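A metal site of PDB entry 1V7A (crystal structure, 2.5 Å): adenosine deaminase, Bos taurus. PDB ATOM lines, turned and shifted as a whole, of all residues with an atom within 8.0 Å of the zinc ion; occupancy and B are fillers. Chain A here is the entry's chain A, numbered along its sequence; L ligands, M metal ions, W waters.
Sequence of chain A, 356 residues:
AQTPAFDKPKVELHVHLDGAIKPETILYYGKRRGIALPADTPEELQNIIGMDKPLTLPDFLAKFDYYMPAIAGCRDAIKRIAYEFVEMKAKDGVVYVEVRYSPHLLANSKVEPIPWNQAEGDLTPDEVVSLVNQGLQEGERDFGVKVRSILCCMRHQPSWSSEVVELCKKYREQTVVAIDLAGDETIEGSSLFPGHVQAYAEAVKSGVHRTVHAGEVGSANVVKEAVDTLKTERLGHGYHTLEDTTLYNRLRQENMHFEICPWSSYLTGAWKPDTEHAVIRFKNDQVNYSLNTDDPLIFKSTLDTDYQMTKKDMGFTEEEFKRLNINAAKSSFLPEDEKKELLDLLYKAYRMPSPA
ND1 of His 14 lies within hydrogen-bond range of NH1 of Arg 100, at 2.8 Å. N of His 16 lies within hydrogen-bond range of O of Asp 294 (2.8 Å). OD1 of Asp 294 sits at hydrogen-bond distance from OG of Ser 264 (2.6 Å). OD1 of Asp 180 is in hydrogen-bond range of ND1 of His 213. The side-chain carboxylate (OE2) of Glu 259 sits at hydrogen-bond distance from a ring nitrogen (ND1) of His 14 (2.9 Å). The backbone NH of His 213 sits at hydrogen-bond distance from the backbone carbonyl oxygen of Leu 181 (2.9 Å). O of His 14 lies within hydrogen-bond range of N of Asp 294 (3.1 Å).
The zinc ion is bound by water W1, a ring nitrogen (NE2) of His 16, a ring nitrogen (NE2) of His 213 and a ring nitrogen (NE2) of His 14. Slightly farther from the zinc ion lies OD2 of Asp 294 (2.7 Å).
The side-chain carboxylate (OD1) of Asp 295 is in hydrogen-bond range of a nitrogen (N2) of the ligand. An oxygen (O2) of the ligand lies within hydrogen-bond range of a ring nitrogen (ND1) of His 16, at 3.1 Å.
Water W1 bridges NE2 of His 237 (2.6 Å) and OD2 of Asp 294 (2.7 Å).
Within 4 Å of the zinc ion: His 14, His 16, His 213 and Asp 294.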
ATOM      1  N   HIS A  14      19.135  17.920 -13.441  1.00  0.00           N
ATOM      2  CA  HIS A  14      20.065  19.024 -13.793  1.00  0.00           C
ATOM      3  C   HIS A  14      20.641  18.944 -15.217  1.00  0.00           C
ATOM      4  O   HIS A  14      21.760  18.508 -15.470  1.00  0.00           O
ATOM      5  CB  HIS A  14      21.243  19.127 -12.812  1.00  0.00           C
ATOM      6  CG  HIS A  14      21.932  20.498 -12.883  1.00  0.00           C
ATOM      7  ND1 HIS A  14      21.943  21.371 -11.874  1.00  0.00           N
ATOM      8  CD2 HIS A  14      22.563  21.103 -13.962  1.00  0.00           C
ATOM      9  CE1 HIS A  14      22.561  22.489 -12.274  1.00  0.00           C
ATOM     10  NE2 HIS A  14      22.934  22.352 -13.596  1.00  0.00           N
ATOM     11  N   VAL A  15      19.814  19.459 -16.126  1.00  0.00           N
ATOM     12  CA  VAL A  15      20.060  19.600 -17.567  1.00  0.00           C
ATOM     13  C   VAL A  15      19.349  20.849 -18.107  1.00  0.00           C
ATOM     14  O   VAL A  15      18.204  21.121 -17.763  1.00  0.00           O
ATOM     15  CB  VAL A  15      19.632  18.346 -18.350  1.00  0.00           C
ATOM     16  CG1 VAL A  15      18.154  18.006 -18.206  1.00  0.00           C
ATOM     17  CG2 VAL A  15      19.963  18.512 -19.846  1.00  0.00           C
ATOM     18  N   HIS A  16      20.084  21.650 -18.885  1.00  0.00           N
ATOM     19  CA  HIS A  16      19.433  22.854 -19.430  1.00  0.00           C
ATOM     20  C   HIS A  16      18.933  22.652 -20.866  1.00  0.00           C
ATOM     21  O   HIS A  16      19.712  22.259 -21.714  1.00  0.00           O
ATOM     22  CB  HIS A  16      20.390  24.056 -19.459  1.00  0.00           C
ATOM     23  CG  HIS A  16      20.998  24.441 -18.110  1.00  0.00           C
ATOM     24  ND1 HIS A  16      20.817  25.634 -17.500  1.00  0.00           N
ATOM     25  CD2 HIS A  16      21.929  23.726 -17.355  1.00  0.00           C
ATOM     26  CE1 HIS A  16      21.599  25.683 -16.410  1.00  0.00           C
ATOM     27  NE2 HIS A  16      22.292  24.501 -16.304  1.00  0.00           N
ATOM     28  N   ARG A 100      15.562  22.139 -16.900  1.00  0.00           N
ATOM     29  CA  ARG A 100      15.462  23.556 -16.549  1.00  0.00           C
ATOM     30  C   ARG A 100      15.911  24.493 -17.642  1.00  0.00           C
ATOM     31  O   ARG A 100      16.702  24.171 -18.539  1.00  0.00           O
ATOM     32  CB  ARG A 100      16.293  23.960 -15.328  1.00  0.00           C
ATOM     33  CG  ARG A 100      17.792  23.719 -15.539  1.00  0.00           C
ATOM     34  CD  ARG A 100      18.225  22.551 -14.674  1.00  0.00           C
ATOM     35  NE  ARG A 100      18.606  23.133 -13.401  1.00  0.00           N
ATOM     36  CZ  ARG A 100      18.752  22.478 -12.276  1.00  0.00           C
ATOM     37  NH1 ARG A 100      19.706  22.969 -11.518  1.00  0.00           N
ATOM     38  NH2 ARG A 100      18.070  21.424 -11.859  1.00  0.00           N
ATOM     39  N   CYS A 152      14.106  29.082 -14.496  1.00  0.00           N
ATOM     40  CA  CYS A 152      15.339  29.666 -13.915  1.00  0.00           C
ATOM     41  C   CYS A 152      15.367  31.169 -13.762  1.00  0.00           C
ATOM     42  O   CYS A 152      15.520  31.876 -14.745  1.00  0.00           O
ATOM     43  CB  CYS A 152      16.572  29.380 -14.746  1.00  0.00           C
ATOM     44  SG  CYS A 152      17.088  27.631 -14.920  1.00  0.00           S
ATOM     45  N   ASP A 180      14.680  27.615 -10.111  1.00  0.00           N
ATOM     46  CA  ASP A 180      16.126  27.582 -10.015  1.00  0.00           C
ATOM     47  C   ASP A 180      16.700  29.003 -10.072  1.00  0.00           C
ATOM     48  O   ASP A 180      16.077  29.972 -10.470  1.00  0.00           O
ATOM     49  CB  ASP A 180      16.667  26.655 -11.100  1.00  0.00           C
ATOM     50  CG  ASP A 180      18.190  26.553 -11.061  1.00  0.00           C
ATOM     51  OD1 ASP A 180      18.814  26.874 -12.075  1.00  0.00           O
ATOM     52  OD2 ASP A 180      18.726  26.180 -10.034  1.00  0.00           O
ATOM     53  N   LEU A 181      17.949  29.069  -9.649  1.00  0.00           N
ATOM     54  CA  LEU A 181      18.727  30.283  -9.785  1.00  0.00           C
ATOM     55  C   LEU A 181      20.011  29.959 -10.520  1.00  0.00           C
ATOM     56  O   LEU A 181      20.815  29.083 -10.167  1.00  0.00           O
ATOM     57  CB  LEU A 181      18.953  30.863  -8.378  1.00  0.00           C
ATOM     58  CG  LEU A 181      19.718  32.202  -8.337  1.00  0.00           C
ATOM     59  CD1 LEU A 181      19.070  33.268  -9.220  1.00  0.00           C
ATOM     60  CD2 LEU A 181      19.791  32.676  -6.881  1.00  0.00           C
ATOM     61  N   ALA A 182      20.142  30.676 -11.624  1.00  0.00           N
ATOM     62  CA  ALA A 182      21.193  30.337 -12.550  1.00  0.00           C
ATOM     63  C   ALA A 182      21.950  31.512 -13.126  1.00  0.00           C
ATOM     64  O   ALA A 182      21.563  32.674 -13.057  1.00  0.00           O
ATOM     65  CB  ALA A 182      20.702  29.410 -13.666  1.00  0.00           C
ATOM     66  N   GLY A 183      23.075  31.086 -13.693  1.00  0.00           N
ATOM     67  CA  GLY A 183      24.140  31.892 -14.298  1.00  0.00           C
ATOM     68  C   GLY A 183      24.946  32.825 -13.389  1.00  0.00           C
ATOM     69  O   GLY A 183      24.428  33.829 -12.943  1.00  0.00           O
ATOM     70  N   VAL A 212      19.018  25.489  -6.480  1.00  0.00           N
ATOM     71  CA  VAL A 212      19.849  26.680  -6.784  1.00  0.00           C
ATOM     72  C   VAL A 212      21.219  26.291  -7.302  1.00  0.00           C
ATOM     73  O   VAL A 212      21.849  25.409  -6.752  1.00  0.00           O
ATOM     74  CB  VAL A 212      20.092  27.621  -5.574  1.00  0.00           C
ATOM     75  CG1 VAL A 212      21.056  28.775  -5.844  1.00  0.00           C
ATOM     76  CG2 VAL A 212      18.868  28.361  -5.028  1.00  0.00           C
ATOM     77  N   HIS A 213      21.735  26.992  -8.309  1.00  0.00           N
ATOM     78  CA  HIS A 213      23.133  26.685  -8.638  1.00  0.00           C
ATOM     79  C   HIS A 213      24.340  26.680  -7.681  1.00  0.00           C
ATOM     80  O   HIS A 213      25.073  25.736  -7.743  1.00  0.00           O
ATOM     81  CB  HIS A 213      23.579  27.285  -9.967  1.00  0.00           C
ATOM     82  CG  HIS A 213      23.089  26.504 -11.151  1.00  0.00           C
ATOM     83  ND1 HIS A 213      21.808  26.401 -11.416  1.00  0.00           N
ATOM     84  CD2 HIS A 213      23.791  25.904 -12.192  1.00  0.00           C
ATOM     85  CE1 HIS A 213      21.661  25.761 -12.610  1.00  0.00           C
ATOM     86  NE2 HIS A 213      22.899  25.429 -13.126  1.00  0.00           N
ATOM     87  N   GLU A 216      29.328  25.280  -7.869  1.00  0.00           N
ATOM     88  CA  GLU A 216      30.234  24.921  -8.978  1.00  0.00           C
ATOM     89  C   GLU A 216      31.472  25.808  -9.126  1.00  0.00           C
ATOM     90  O   GLU A 216      32.570  25.354  -9.332  1.00  0.00           O
ATOM     91  CB  GLU A 216      29.404  24.937 -10.242  1.00  0.00           C
ATOM     92  CG  GLU A 216      30.109  25.016 -11.593  1.00  0.00           C
ATOM     93  CD  GLU A 216      29.035  25.273 -12.621  1.00  0.00           C
ATOM     94  OE1 GLU A 216      28.280  26.216 -12.446  1.00  0.00           O
ATOM     95  OE2 GLU A 216      28.934  24.536 -13.601  1.00  0.00           O
ATOM     96  N   GLY A 236      22.428  22.814  -7.063  1.00  0.00           N
ATOM     97  CA  GLY A 236      23.022  22.511  -8.360  1.00  0.00           C
ATOM     98  C   GLY A 236      24.540  22.486  -8.384  1.00  0.00           C
ATOM     99  O   GLY A 236      25.216  23.480  -8.233  1.00  0.00           O
ATOM    100  N   HIS A 237      25.081  21.308  -8.586  1.00  0.00           N
ATOM    101  CA  HIS A 237      26.513  21.086  -8.318  1.00  0.00           C
ATOM    102  C   HIS A 237      26.902  21.026  -6.848  1.00  0.00           C
ATOM    103  O   HIS A 237      27.199  19.978  -6.297  1.00  0.00           O
ATOM    104  CB  HIS A 237      27.523  22.046  -8.942  1.00  0.00           C
ATOM    105  CG  HIS A 237      27.314  22.224 -10.438  1.00  0.00           C
ATOM    106  ND1 HIS A 237      28.039  21.590 -11.377  1.00  0.00           N
ATOM    107  CD2 HIS A 237      26.405  23.063 -11.064  1.00  0.00           C
ATOM    108  CE1 HIS A 237      27.620  21.974 -12.591  1.00  0.00           C
ATOM    109  NE2 HIS A 237      26.633  22.880 -12.364  1.00  0.00           N
ATOM    110  N   GLU A 259      23.080  18.038  -7.046  1.00  0.00           N
ATOM    111  CA  GLU A 259      23.055  17.823  -8.491  1.00  0.00           C
ATOM    112  C   GLU A 259      24.421  17.752  -9.178  1.00  0.00           C
ATOM    113  O   GLU A 259      24.929  18.748  -9.686  1.00  0.00           O
ATOM    114  CB  GLU A 259      22.134  18.857  -9.156  1.00  0.00           C
ATOM    115  CG  GLU A 259      21.003  19.269  -8.190  1.00  0.00           C
ATOM    116  CD  GLU A 259      19.910  20.070  -8.815  1.00  0.00           C
ATOM    117  OE1 GLU A 259      18.766  19.871  -8.467  1.00  0.00           O
ATOM    118  OE2 GLU A 259      20.197  20.901  -9.645  1.00  0.00           O
ATOM    119  N   CYS A 261      27.490  17.164 -11.690  1.00  0.00           N
ATOM    120  CA  CYS A 261      27.717  17.048 -13.110  1.00  0.00           C
ATOM    121  C   CYS A 261      29.185  16.833 -13.454  1.00  0.00           C
ATOM    122  O   CYS A 261      29.908  17.799 -13.689  1.00  0.00           O
ATOM    123  CB  CYS A 261      27.269  18.334 -13.804  1.00  0.00           C
ATOM    124  SG  CYS A 261      25.578  18.941 -13.488  1.00  0.00           S
ATOM    125  N   SER A 264      30.494  18.007 -17.222  1.00  0.00           N
ATOM    126  CA  SER A 264      30.420  19.463 -17.016  1.00  0.00           C
ATOM    127  C   SER A 264      31.529  20.105 -16.198  1.00  0.00           C
ATOM    128  O   SER A 264      32.101  21.105 -16.594  1.00  0.00           O
ATOM    129  CB  SER A 264      29.121  19.917 -16.345  1.00  0.00           C
ATOM    130  OG  SER A 264      29.052  21.374 -16.341  1.00  0.00           O
ATOM    131  N   THR A 293      23.959  15.695 -16.771  1.00  0.00           N
ATOM    132  CA  THR A 293      24.557  16.107 -18.052  1.00  0.00           C
ATOM    133  C   THR A 293      24.960  17.609 -18.130  1.00  0.00           C
ATOM    134  O   THR A 293      25.921  18.050 -18.762  1.00  0.00           O
ATOM    135  CB  THR A 293      23.550  15.606 -19.120  1.00  0.00           C
ATOM    136  OG1 THR A 293      23.950  14.487 -19.902  1.00  0.00           O
ATOM    137  CG2 THR A 293      22.999  16.754 -19.910  1.00  0.00           C
ATOM    138  N   ASP A 294      24.118  18.405 -17.466  1.00  0.00           N
ATOM    139  CA  ASP A 294      24.187  19.855 -17.571  1.00  0.00           C
ATOM    140  C   ASP A 294      23.841  20.508 -18.908  1.00  0.00           C
ATOM    141  O   ASP A 294      22.843  21.208 -19.024  1.00  0.00           O
ATOM    142  CB  ASP A 294      25.514  20.301 -17.033  1.00  0.00           C
ATOM    143  CG  ASP A 294      25.473  21.603 -16.311  1.00  0.00           C
ATOM    144  OD1 ASP A 294      26.527  21.969 -15.807  1.00  0.00           O
ATOM    145  OD2 ASP A 294      24.422  22.245 -16.259  1.00  0.00           O
ATOM    146  N   ASP A 295      24.728  20.317 -19.898  1.00  0.00           N
ATOM    147  CA  ASP A 295      24.562  20.915 -21.249  1.00  0.00           C
ATOM    148  C   ASP A 295      25.215  20.087 -22.366  1.00  0.00           C
ATOM    149  O   ASP A 295      26.368  20.325 -22.723  1.00  0.00           O
ATOM    150  CB  ASP A 295      25.265  22.281 -21.361  1.00  0.00           C
ATOM    151  CG  ASP A 295      24.888  23.272 -20.279  1.00  0.00           C
ATOM    152  OD1 ASP A 295      24.048  24.116 -20.543  1.00  0.00           O
ATOM    153  OD2 ASP A 295      25.463  23.202 -19.195  1.00  0.00           O
ATOM    154  N   PHE A 299      28.834  20.652 -23.937  1.00  0.00           N
ATOM    155  CA  PHE A 299      29.883  19.769 -23.432  1.00  0.00           C
ATOM    156  C   PHE A 299      30.193  18.559 -24.341  1.00  0.00           C
ATOM    157  O   PHE A 299      30.910  17.640 -23.968  1.00  0.00           O
ATOM    158  CB  PHE A 299      29.544  19.363 -21.973  1.00  0.00           C
ATOM    159  CG  PHE A 299      29.394  20.556 -21.052  1.00  0.00           C
ATOM    160  CD1 PHE A 299      30.317  21.625 -21.042  1.00  0.00           C
ATOM    161  CD2 PHE A 299      28.294  20.576 -20.156  1.00  0.00           C
ATOM    162  CE1 PHE A 299      30.190  22.682 -20.121  1.00  0.00           C
ATOM    163  CE2 PHE A 299      28.153  21.635 -19.233  1.00  0.00           C
ATOM    164  CZ  PHE A 299      29.109  22.678 -19.223  1.00  0.00           C
HETATM  165  C1  LIG L   1      22.825  28.326 -18.113  1.00  0.00           C
HETATM  166  N1  LIG L   1      21.874  28.184 -19.214  1.00  0.00           N
HETATM  167  C2  LIG L   1      22.232  27.135 -19.951  1.00  0.00           C
HETATM  168  N2  LIG L   1      23.261  26.474 -19.385  1.00  0.00           N
HETATM  169  C3  LIG L   1      23.716  27.339 -18.274  1.00  0.00           C
HETATM  170  C4  LIG L   1      24.973  27.164 -17.508  1.00  0.00           C
HETATM  171  O1  LIG L   1      25.337  27.941 -16.644  1.00  0.00           O
HETATM  172  N3  LIG L   1      25.689  26.078 -17.779  1.00  0.00           N
HETATM  173  C5  LIG L   1      20.791  29.090 -19.531  1.00  0.00           C
HETATM  174  C6  LIG L   1      19.520  28.751 -18.716  1.00  0.00           C
HETATM  175  O2  LIG L   1      18.878  27.462 -19.042  1.00  0.00           O
HETATM  176  C7  LIG L   1      21.221  30.556 -19.454  1.00  0.00           C
HETATM  177  C8  LIG L   1      21.996  30.920 -20.728  1.00  0.00           C
HETATM  178  C9  LIG L   1      19.742  29.113 -17.219  1.00  0.00           C
HETATM  179  O3  LIG L   1      22.465  32.253 -20.683  1.00  0.00           O
HETATM  180  C10 LIG L   1      26.985  32.945 -16.187  1.00  0.00           C
HETATM  181  C11 LIG L   1      26.169  33.872 -16.857  1.00  0.00           C
HETATM  182  C12 LIG L   1      25.207  33.417 -17.749  1.00  0.00           C
HETATM  183  C13 LIG L   1      25.118  32.041 -18.057  1.00  0.00           C
HETATM  184  C14 LIG L   1      25.921  31.121 -17.377  1.00  0.00           C
HETATM  185  C15 LIG L   1      26.867  31.574 -16.452  1.00  0.00           C
HETATM  186  C16 LIG L   1      24.425  34.358 -18.440  1.00  0.00           C
HETATM  187  C17 LIG L   1      23.517  33.888 -19.387  1.00  0.00           C
HETATM  188  C18 LIG L   1      23.399  32.526 -19.699  1.00  0.00           C
HETATM  189  C19 LIG L   1      24.195  31.584 -19.011  1.00  0.00           C
HETATM  190 ZN    ZN M   1      23.255  24.092 -14.644  1.00  0.00          ZN
HETATM  191  O   HOH W   1      25.148  23.841 -14.223  1.00  0.00           O
